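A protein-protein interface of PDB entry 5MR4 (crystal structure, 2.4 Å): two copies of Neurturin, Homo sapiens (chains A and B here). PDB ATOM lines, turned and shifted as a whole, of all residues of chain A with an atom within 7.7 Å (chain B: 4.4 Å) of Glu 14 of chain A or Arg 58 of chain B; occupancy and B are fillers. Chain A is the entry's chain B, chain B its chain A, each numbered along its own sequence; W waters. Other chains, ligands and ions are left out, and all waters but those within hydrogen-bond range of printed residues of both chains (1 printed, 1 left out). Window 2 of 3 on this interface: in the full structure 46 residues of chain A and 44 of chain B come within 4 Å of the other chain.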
ATOM      1  N   GLU A  12      -5.979  -7.374 -12.858  1.00  0.00           N
ATOM      2  CA  GLU A  12      -4.931  -6.742 -13.660  1.00  0.00           C
ATOM      3  C   GLU A  12      -5.449  -6.457 -15.029  1.00  0.00           C
ATOM      4  O   GLU A  12      -6.216  -7.219 -15.571  1.00  0.00           O
ATOM      5  CB  GLU A  12      -3.746  -7.662 -13.838  1.00  0.00           C
ATOM      6  CG  GLU A  12      -2.782  -7.672 -12.675  1.00  0.00           C
ATOM      7  CD  GLU A  12      -1.693  -8.693 -12.852  1.00  0.00           C
ATOM      8  OE1 GLU A  12      -1.095  -9.098 -11.827  1.00  0.00           O
ATOM      9  OE2 GLU A  12      -1.450  -9.091 -14.008  1.00  0.00           O
ATOM     10  N   LEU A  13      -4.991  -5.363 -15.601  1.00  0.00           N
ATOM     11  CA  LEU A  13      -5.418  -4.954 -16.917  1.00  0.00           C
ATOM     12  C   LEU A  13      -4.311  -4.080 -17.499  1.00  0.00           C
ATOM     13  O   LEU A  13      -3.823  -3.164 -16.832  1.00  0.00           O
ATOM     14  CB  LEU A  13      -6.693  -4.164 -16.784  1.00  0.00           C
ATOM     15  CG  LEU A  13      -7.327  -3.674 -18.064  1.00  0.00           C
ATOM     16  CD1 LEU A  13      -7.862  -4.878 -18.825  1.00  0.00           C
ATOM     17  CD2 LEU A  13      -8.447  -2.715 -17.719  1.00  0.00           C
ATOM     18  N   GLU A  14      -3.881  -4.404 -18.711  1.00  0.00           N
ATOM     19  CA  GLU A  14      -2.947  -3.578 -19.438  1.00  0.00           C
ATOM     20  C   GLU A  14      -3.738  -2.431 -20.053  1.00  0.00           C
ATOM     21  O   GLU A  14      -4.681  -2.670 -20.791  1.00  0.00           O
ATOM     22  CB  GLU A  14      -2.258  -4.376 -20.551  1.00  0.00           C
ATOM     23  CG  GLU A  14      -1.407  -5.521 -20.033  1.00  0.00           C
ATOM     24  CD  GLU A  14      -0.605  -6.264 -21.118  1.00  0.00           C
ATOM     25  OE1 GLU A  14      -0.059  -7.350 -20.787  1.00  0.00           O
ATOM     26  OE2 GLU A  14      -0.506  -5.782 -22.274  1.00  0.00           O
ATOM     27  N   VAL A  15      -3.356  -1.193 -19.744  1.00  0.00           N
ATOM     28  CA  VAL A  15      -4.013  -0.037 -20.300  1.00  0.00           C
ATOM     29  C   VAL A  15      -3.020   0.930 -20.895  1.00  0.00           C
ATOM     30  O   VAL A  15      -1.896   1.071 -20.423  1.00  0.00           O
ATOM     31  CB  VAL A  15      -4.862   0.707 -19.246  1.00  0.00           C
ATOM     32  CG1 VAL A  15      -5.884  -0.237 -18.640  1.00  0.00           C
ATOM     33  CG2 VAL A  15      -4.002   1.294 -18.139  1.00  0.00           C
ATOM     34  N   ARG A  16      -3.464   1.604 -21.927  1.00  0.00           N
ATOM     35  CA  ARG A  16      -2.736   2.719 -22.502  1.00  0.00           C
ATOM     36  C   ARG A  16      -3.010   3.917 -21.600  1.00  0.00           C
ATOM     37  O   ARG A  16      -4.163   4.162 -21.255  1.00  0.00           O
ATOM     38  CB  ARG A  16      -3.229   2.981 -23.934  1.00  0.00           C
ATOM     39  CG  ARG A  16      -2.114   3.309 -24.919  1.00  0.00           C
ATOM     40  CD  ARG A  16      -2.633   3.539 -26.338  1.00  0.00           C
ATOM     41  NE  ARG A  16      -3.232   2.324 -26.890  1.00  0.00           N
ATOM     42  CZ  ARG A  16      -2.560   1.254 -27.336  1.00  0.00           C
ATOM     43  NH1 ARG A  16      -1.223   1.207 -27.311  1.00  0.00           N
ATOM     44  NH2 ARG A  16      -3.241   0.205 -27.808  1.00  0.00           N
ATOM     45  N   VAL A  17      -1.990   4.684 -21.230  1.00  0.00           N
ATOM     46  CA  VAL A  17      -2.202   5.735 -20.232  1.00  0.00           C
ATOM     47  C   VAL A  17      -3.168   6.803 -20.727  1.00  0.00           C
ATOM     48  O   VAL A  17      -3.886   7.389 -19.932  1.00  0.00           O
ATOM     49  CB  VAL A  17      -0.914   6.367 -19.612  1.00  0.00           C
ATOM     50  CG1 VAL A  17       0.171   5.344 -19.343  1.00  0.00           C
ATOM     51  CG2 VAL A  17      -0.349   7.432 -20.472  1.00  0.00           C
ATOM     52  N   GLU A  19      -5.903   6.243 -22.309  1.00  0.00           N
ATOM     53  CA  GLU A  19      -7.276   5.758 -22.114  1.00  0.00           C
ATOM     54  C   GLU A  19      -7.852   6.133 -20.737  1.00  0.00           C
ATOM     55  O   GLU A  19      -9.060   6.053 -20.551  1.00  0.00           O
ATOM     56  CB  GLU A  19      -7.349   4.225 -22.143  1.00  0.00           C
ATOM     57  CG  GLU A  19      -7.017   3.464 -23.412  1.00  0.00           C
ATOM     58  CD  GLU A  19      -6.840   1.952 -23.086  1.00  0.00           C
ATOM     59  OE1 GLU A  19      -7.500   1.474 -22.123  1.00  0.00           O
ATOM     60  OE2 GLU A  19      -6.036   1.233 -23.751  1.00  0.00           O
ATOM     61  N   THR A  29       2.058   2.009 -21.992  1.00  0.00           N
ATOM     62  CA  THR A  29       1.115   1.180 -21.266  1.00  0.00           C
ATOM     63  C   THR A  29       1.531   0.999 -19.819  1.00  0.00           C
ATOM     64  O   THR A  29       2.722   0.992 -19.485  1.00  0.00           O
ATOM     65  CB  THR A  29       0.811  -0.195 -21.926  1.00  0.00           C
ATOM     66  OG1 THR A  29       1.627  -1.212 -21.372  1.00  0.00           O
ATOM     67  CG2 THR A  29       1.009  -0.176 -23.356  1.00  0.00           C
ATOM     68  N   VAL A  30       0.529   0.851 -18.959  1.00  0.00           N
ATOM     69  CA  VAL A  30       0.783   0.510 -17.554  1.00  0.00           C
ATOM     70  C   VAL A  30      -0.018  -0.728 -17.209  1.00  0.00           C
ATOM     71  O   VAL A  30      -1.036  -1.019 -17.856  1.00  0.00           O
ATOM     72  CB  VAL A  30       0.471   1.687 -16.590  1.00  0.00           C
ATOM     73  CG1 VAL A  30       1.370   2.877 -16.902  1.00  0.00           C
ATOM     74  CG2 VAL A  30      -0.979   2.117 -16.669  1.00  0.00           C
ATOM     75  N   LEU A  31       0.457  -1.475 -16.225  1.00  0.00           N
ATOM     76  CA  LEU A  31      -0.329  -2.544 -15.653  1.00  0.00           C
ATOM     77  C   LEU A  31      -1.192  -1.918 -14.581  1.00  0.00           C
ATOM     78  O   LEU A  31      -0.720  -1.578 -13.519  1.00  0.00           O
ATOM     79  CB  LEU A  31       0.567  -3.600 -15.043  1.00  0.00           C
ATOM     80  CG  LEU A  31      -0.078  -4.952 -14.691  1.00  0.00           C
ATOM     81  CD1 LEU A  31      -0.675  -5.674 -15.895  1.00  0.00           C
ATOM     82  CD2 LEU A  31       0.968  -5.842 -14.062  1.00  0.00           C
ATOM     83  N   PHE A  32      -2.461  -1.726 -14.883  1.00  0.00           N
ATOM     84  CA  PHE A  32      -3.405  -1.233 -13.912  1.00  0.00           C
ATOM     85  C   PHE A  32      -3.992  -2.370 -13.078  1.00  0.00           C
ATOM     86  O   PHE A  32      -4.664  -3.223 -13.616  1.00  0.00           O
ATOM     87  CB  PHE A  32      -4.506  -0.498 -14.650  1.00  0.00           C
ATOM     88  CG  PHE A  32      -5.506   0.147 -13.761  1.00  0.00           C
ATOM     89  CD1 PHE A  32      -5.209   1.317 -13.099  1.00  0.00           C
ATOM     90  CD2 PHE A  32      -6.771  -0.399 -13.615  1.00  0.00           C
ATOM     91  CE1 PHE A  32      -6.152   1.932 -12.287  1.00  0.00           C
ATOM     92  CE2 PHE A  32      -7.717   0.205 -12.801  1.00  0.00           C
ATOM     93  CZ  PHE A  32      -7.406   1.370 -12.140  1.00  0.00           C
ATOM     94  N   ARG A  33      -3.743  -2.355 -11.775  1.00  0.00           N
ATOM     95  CA  ARG A  33      -4.341  -3.302 -10.818  1.00  0.00           C
ATOM     96  C   ARG A  33      -5.456  -2.667 -10.003  1.00  0.00           C
ATOM     97  O   ARG A  33      -5.336  -1.527  -9.565  1.00  0.00           O
ATOM     98  CB  ARG A  33      -3.300  -3.808  -9.826  1.00  0.00           C
ATOM     99  CG  ARG A  33      -2.133  -4.516 -10.481  1.00  0.00           C
ATOM    100  CD  ARG A  33      -1.523  -5.595  -9.606  1.00  0.00           C
ATOM    101  NE  ARG A  33      -0.387  -6.161 -10.316  1.00  0.00           N
ATOM    102  CZ  ARG A  33       0.885  -5.799 -10.152  1.00  0.00           C
ATOM    103  NH1 ARG A  33       1.226  -4.891  -9.244  1.00  0.00           N
ATOM    104  NH2 ARG A  33       1.831  -6.370 -10.885  1.00  0.00           N
ATOM    105  N   TYR A  34      -6.509  -3.432  -9.744  1.00  0.00           N
ATOM    106  CA  TYR A  34      -7.637  -2.935  -8.986  1.00  0.00           C
ATOM    107  C   TYR A  34      -8.270  -4.037  -8.171  1.00  0.00           C
ATOM    108  O   TYR A  34      -7.942  -5.200  -8.347  1.00  0.00           O
ATOM    109  CB  TYR A  34      -8.655  -2.314  -9.924  1.00  0.00           C
ATOM    110  CG  TYR A  34      -9.225  -3.257 -10.966  1.00  0.00           C
ATOM    111  CD1 TYR A  34      -8.523  -3.554 -12.132  1.00  0.00           C
ATOM    112  CD2 TYR A  34     -10.496  -3.813 -10.814  1.00  0.00           C
ATOM    113  CE1 TYR A  34      -9.059  -4.393 -13.101  1.00  0.00           C
ATOM    114  CE2 TYR A  34     -11.032  -4.642 -11.780  1.00  0.00           C
ATOM    115  CZ  TYR A  34     -10.301  -4.936 -12.916  1.00  0.00           C
ATOM    116  OH  TYR A  34     -10.836  -5.767 -13.865  1.00  0.00           O
ATOM    117  N   LEU B  53     -12.417   3.376 -16.960  1.00  0.00           N
ATOM    118  CA  LEU B  53     -12.342   2.027 -17.459  1.00  0.00           C
ATOM    119  C   LEU B  53     -13.674   1.259 -17.381  1.00  0.00           C
ATOM    120  O   LEU B  53     -14.007   0.509 -18.292  1.00  0.00           O
ATOM    121  CB  LEU B  53     -11.273   1.251 -16.717  1.00  0.00           C
ATOM    122  CG  LEU B  53      -9.842   1.699 -16.973  1.00  0.00           C
ATOM    123  CD1 LEU B  53      -8.912   0.996 -16.005  1.00  0.00           C
ATOM    124  CD2 LEU B  53      -9.437   1.409 -18.408  1.00  0.00           C
ATOM    125  N   ARG B  56     -16.021   2.668 -20.062  1.00  0.00           N
ATOM    126  CA  ARG B  56     -15.515   2.149 -21.318  1.00  0.00           C
ATOM    127  C   ARG B  56     -15.664   0.626 -21.443  1.00  0.00           C
ATOM    128  O   ARG B  56     -15.266   0.053 -22.437  1.00  0.00           O
ATOM    129  CB  ARG B  56     -14.040   2.533 -21.472  1.00  0.00           C
ATOM    130  CG  ARG B  56     -13.759   3.243 -22.772  1.00  0.00           C
ATOM    131  CD  ARG B  56     -14.147   4.706 -22.707  1.00  0.00           C
ATOM    132  NE  ARG B  56     -13.325   5.520 -23.605  1.00  0.00           N
ATOM    133  CZ  ARG B  56     -12.005   5.716 -23.468  1.00  0.00           C
ATOM    134  NH1 ARG B  56     -11.363   6.498 -24.327  1.00  0.00           N
ATOM    135  NH2 ARG B  56     -11.304   5.123 -22.485  1.00  0.00           N
ATOM    136  N   ARG B  57     -16.205  -0.020 -20.418  1.00  0.00           N
ATOM    137  CA  ARG B  57     -16.460  -1.460 -20.419  1.00  0.00           C
ATOM    138  C   ARG B  57     -15.175  -2.252 -20.600  1.00  0.00           C
ATOM    139  O   ARG B  57     -15.147  -3.261 -21.284  1.00  0.00           O
ATOM    140  CB  ARG B  57     -17.474  -1.851 -21.510  1.00  0.00           C
ATOM    141  CG  ARG B  57     -18.728  -0.996 -21.547  1.00  0.00           C
ATOM    142  CD  ARG B  57     -19.935  -1.728 -21.002  1.00  0.00           C
ATOM    143  NE  ARG B  57     -21.045  -1.704 -21.951  1.00  0.00           N
ATOM    144  CZ  ARG B  57     -22.167  -2.413 -21.829  1.00  0.00           C
ATOM    145  NH1 ARG B  57     -22.362  -3.215 -20.783  1.00  0.00           N
ATOM    146  NH2 ARG B  57     -23.109  -2.319 -22.766  1.00  0.00           N
ATOM    147  N   ARG B  58     -14.109  -1.793 -19.974  1.00  0.00           N
ATOM    148  CA  ARG B  58     -12.811  -2.472 -20.046  1.00  0.00           C
ATOM    149  C   ARG B  58     -12.677  -3.513 -18.944  1.00  0.00           C
ATOM    150  O   ARG B  58     -11.741  -4.298 -18.937  1.00  0.00           O
ATOM    151  CB  ARG B  58     -11.665  -1.458 -19.942  1.00  0.00           C
ATOM    152  CG  ARG B  58     -11.501  -0.600 -21.183  1.00  0.00           C
ATOM    153  CD  ARG B  58     -10.742  -1.318 -22.300  1.00  0.00           C
ATOM    154  NE  ARG B  58      -9.282  -1.130 -22.191  1.00  0.00           N
ATOM    155  CZ  ARG B  58      -8.400  -2.087 -21.910  1.00  0.00           C
ATOM    156  NH1 ARG B  58      -7.106  -1.787 -21.816  1.00  0.00           N
ATOM    157  NH2 ARG B  58      -8.788  -3.345 -21.723  1.00  0.00           N
ATOM    158  N   LEU B  59     -13.594  -3.507 -18.001  1.00  0.00           N
ATOM    159  CA  LEU B  59     -13.598  -4.490 -16.928  1.00  0.00           C
ATOM    160  C   LEU B  59     -14.363  -5.724 -17.348  1.00  0.00           C
ATOM    161  O   LEU B  59     -15.156  -5.688 -18.293  1.00  0.00           O
ATOM    162  CB  LEU B  59     -14.243  -3.896 -15.673  1.00  0.00           C
ATOM    163  CG  LEU B  59     -13.371  -2.988 -14.785  1.00  0.00           C
ATOM    164  CD1 LEU B  59     -12.229  -2.305 -15.499  1.00  0.00           C
ATOM    165  CD2 LEU B  59     -14.220  -1.947 -14.088  1.00  0.00           C
ATOM    166  N   ARG B  60     -14.171  -6.799 -16.606  1.00  0.00           N
ATOM    167  CA  ARG B  60     -14.714  -8.115 -16.998  1.00  0.00           C
ATOM    168  C   ARG B  60     -16.079  -8.348 -16.353  1.00  0.00           C
ATOM    169  O   ARG B  60     -16.330  -9.401 -15.789  1.00  0.00           O
ATOM    170  CB  ARG B  60     -13.728  -9.263 -16.686  1.00  0.00           C
ATOM    171  CG  ARG B  60     -12.745  -8.964 -15.572  1.00  0.00           C
ATOM    172  CD  ARG B  60     -11.760 -10.094 -15.379  1.00  0.00           C
ATOM    173  NE  ARG B  60     -10.461  -9.595 -14.943  1.00  0.00           N
ATOM    174  CZ  ARG B  60      -9.418 -10.363 -14.650  1.00  0.00           C
ATOM    175  NH1 ARG B  60      -8.287  -9.797 -14.272  1.00  0.00           N
ATOM    176  NH2 ARG B  60      -9.496 -11.689 -14.743  1.00  0.00           N
HETATM  177  O   HOH W   1     -10.174   2.149 -23.042  1.00  0.00           O
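Printed residues of chain A that touch a printed residue of chain B: Glu 12, Leu 13, Glu 14, Val 15, Glu 19, Phe 32 and Tyr 34.
Hydrophobic or aromatic side chains of chain A that line the printed part of chain B: Leu 13, Val 15, Phe 32 and Tyr 34.
Of the 6 printed residues of chain B, 5 touch a printed residue of chain A.
Hydrophobic or aromatic side chains of chain B that line the printed part of chain A: Leu 53 and Leu 59.
Among the printed residues, 10 pairs touch across the chains.
Among the printed residues, Asp or Glu carboxylates within 4 Å of a Lys or Arg side-chain nitrogen of the other chain: Glu 19 of chain A with Arg 58 of chain B (3.2 Å).
Water W1 bridges the side-chain carboxylate (OE1) of Glu 19 of chain A (2.9 Å) and the guanidinium group (NH2) of Arg 56 of chain B (3.2 Å).
No position is printed for both chains.
Of the 10 pairs that touch across the chains among the printed residues, none has its exchanged pair printed and touching as well.
The backbone NH (N) of Arg 58 of chain B lies within hydrogen-bond range of the backbone carbonyl oxygen (O) of Leu 53 of chain B, at 2.9 Å.
The side-chain carboxylate (OE1) of Glu 12 of chain A lies within salt-bridge range of the guanidinium group (NE) of Arg 33 of chain A (3.4 Å).
N of Phe 32 of chain A lies within hydrogen-bond range of O of Leu 13 of chain A (2.8 Å).
The backbone carbonyl oxygen (O) of Val 15 of chain A is in hydrogen-bond range of the backbone NH (N) of Val 30 of chain A (2.8 Å).
N of Arg 16 of chain A sits at hydrogen-bond distance from OE2 of Glu 19 of chain A (3.2 Å).
Of the printed residues of chain B, Glu 12 of chain A touches Arg 60.
Of the printed residues of chain B, Leu 13 of chain A touches Arg 58.
Glu 14 of chain A touches one residue of chain B.
Arg 16 of chain A touches none of the printed residues of chain B.
Printed residues of chain B within 4 Å of Glu 19 of chain A: Arg 56 and Arg 58.
Of chain A, only Leu 13 (3.4 Å), Glu 14 (2.8 Å), Val 15 (3.7 Å) and Glu 19 (3.2 Å) come within 4 Å of Arg 58 of chain B.
The nearest printed residue of chain B that does not touch Glu 14 of chain A is Leu 53 of chain B (6.7 Å).
The nearest printed residue of chain B that does not touch Val 15 of chain A is Leu 59 of chain B (7.4 Å).
O of Glu 19 of chain A lies within hydrogen-bond range of NH2 of Arg 56 of chain B (3.1 Å).
O of Glu 14 of chain A sits at hydrogen-bond distance from NH1 of Arg 58 of chain B (2.8 Å).
The guanidinium group (NE) of Arg 58 of chain B lies within salt-bridge range of the side-chain carboxylate (OE1) of Glu 19 of chain A, 3.2 Å away.
Arg 60 of chain B touches Glu 12 of chain A (NH1 to O, 3.6 Å).
NH2 of Arg 58 of chain B touches CD1 of Leu 13 of chain A, 3.4 Å away.
CD2 of Leu 53 of chain B touches CG1 of Val 15 of chain A, at 3.9 Å.
Val 15 of chain A touches Arg 58 of chain B (CG1 to NH1, 3.7 Å).
Leu 53 of chain B touches Phe 32 of chain A.
Tyr 34 of chain A touches Leu 59 of chain B (OH to CG, 3.9 Å).
Tyr 34 of chain A touches Arg 60 of chain B (OH to NE, 3.99 Å).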
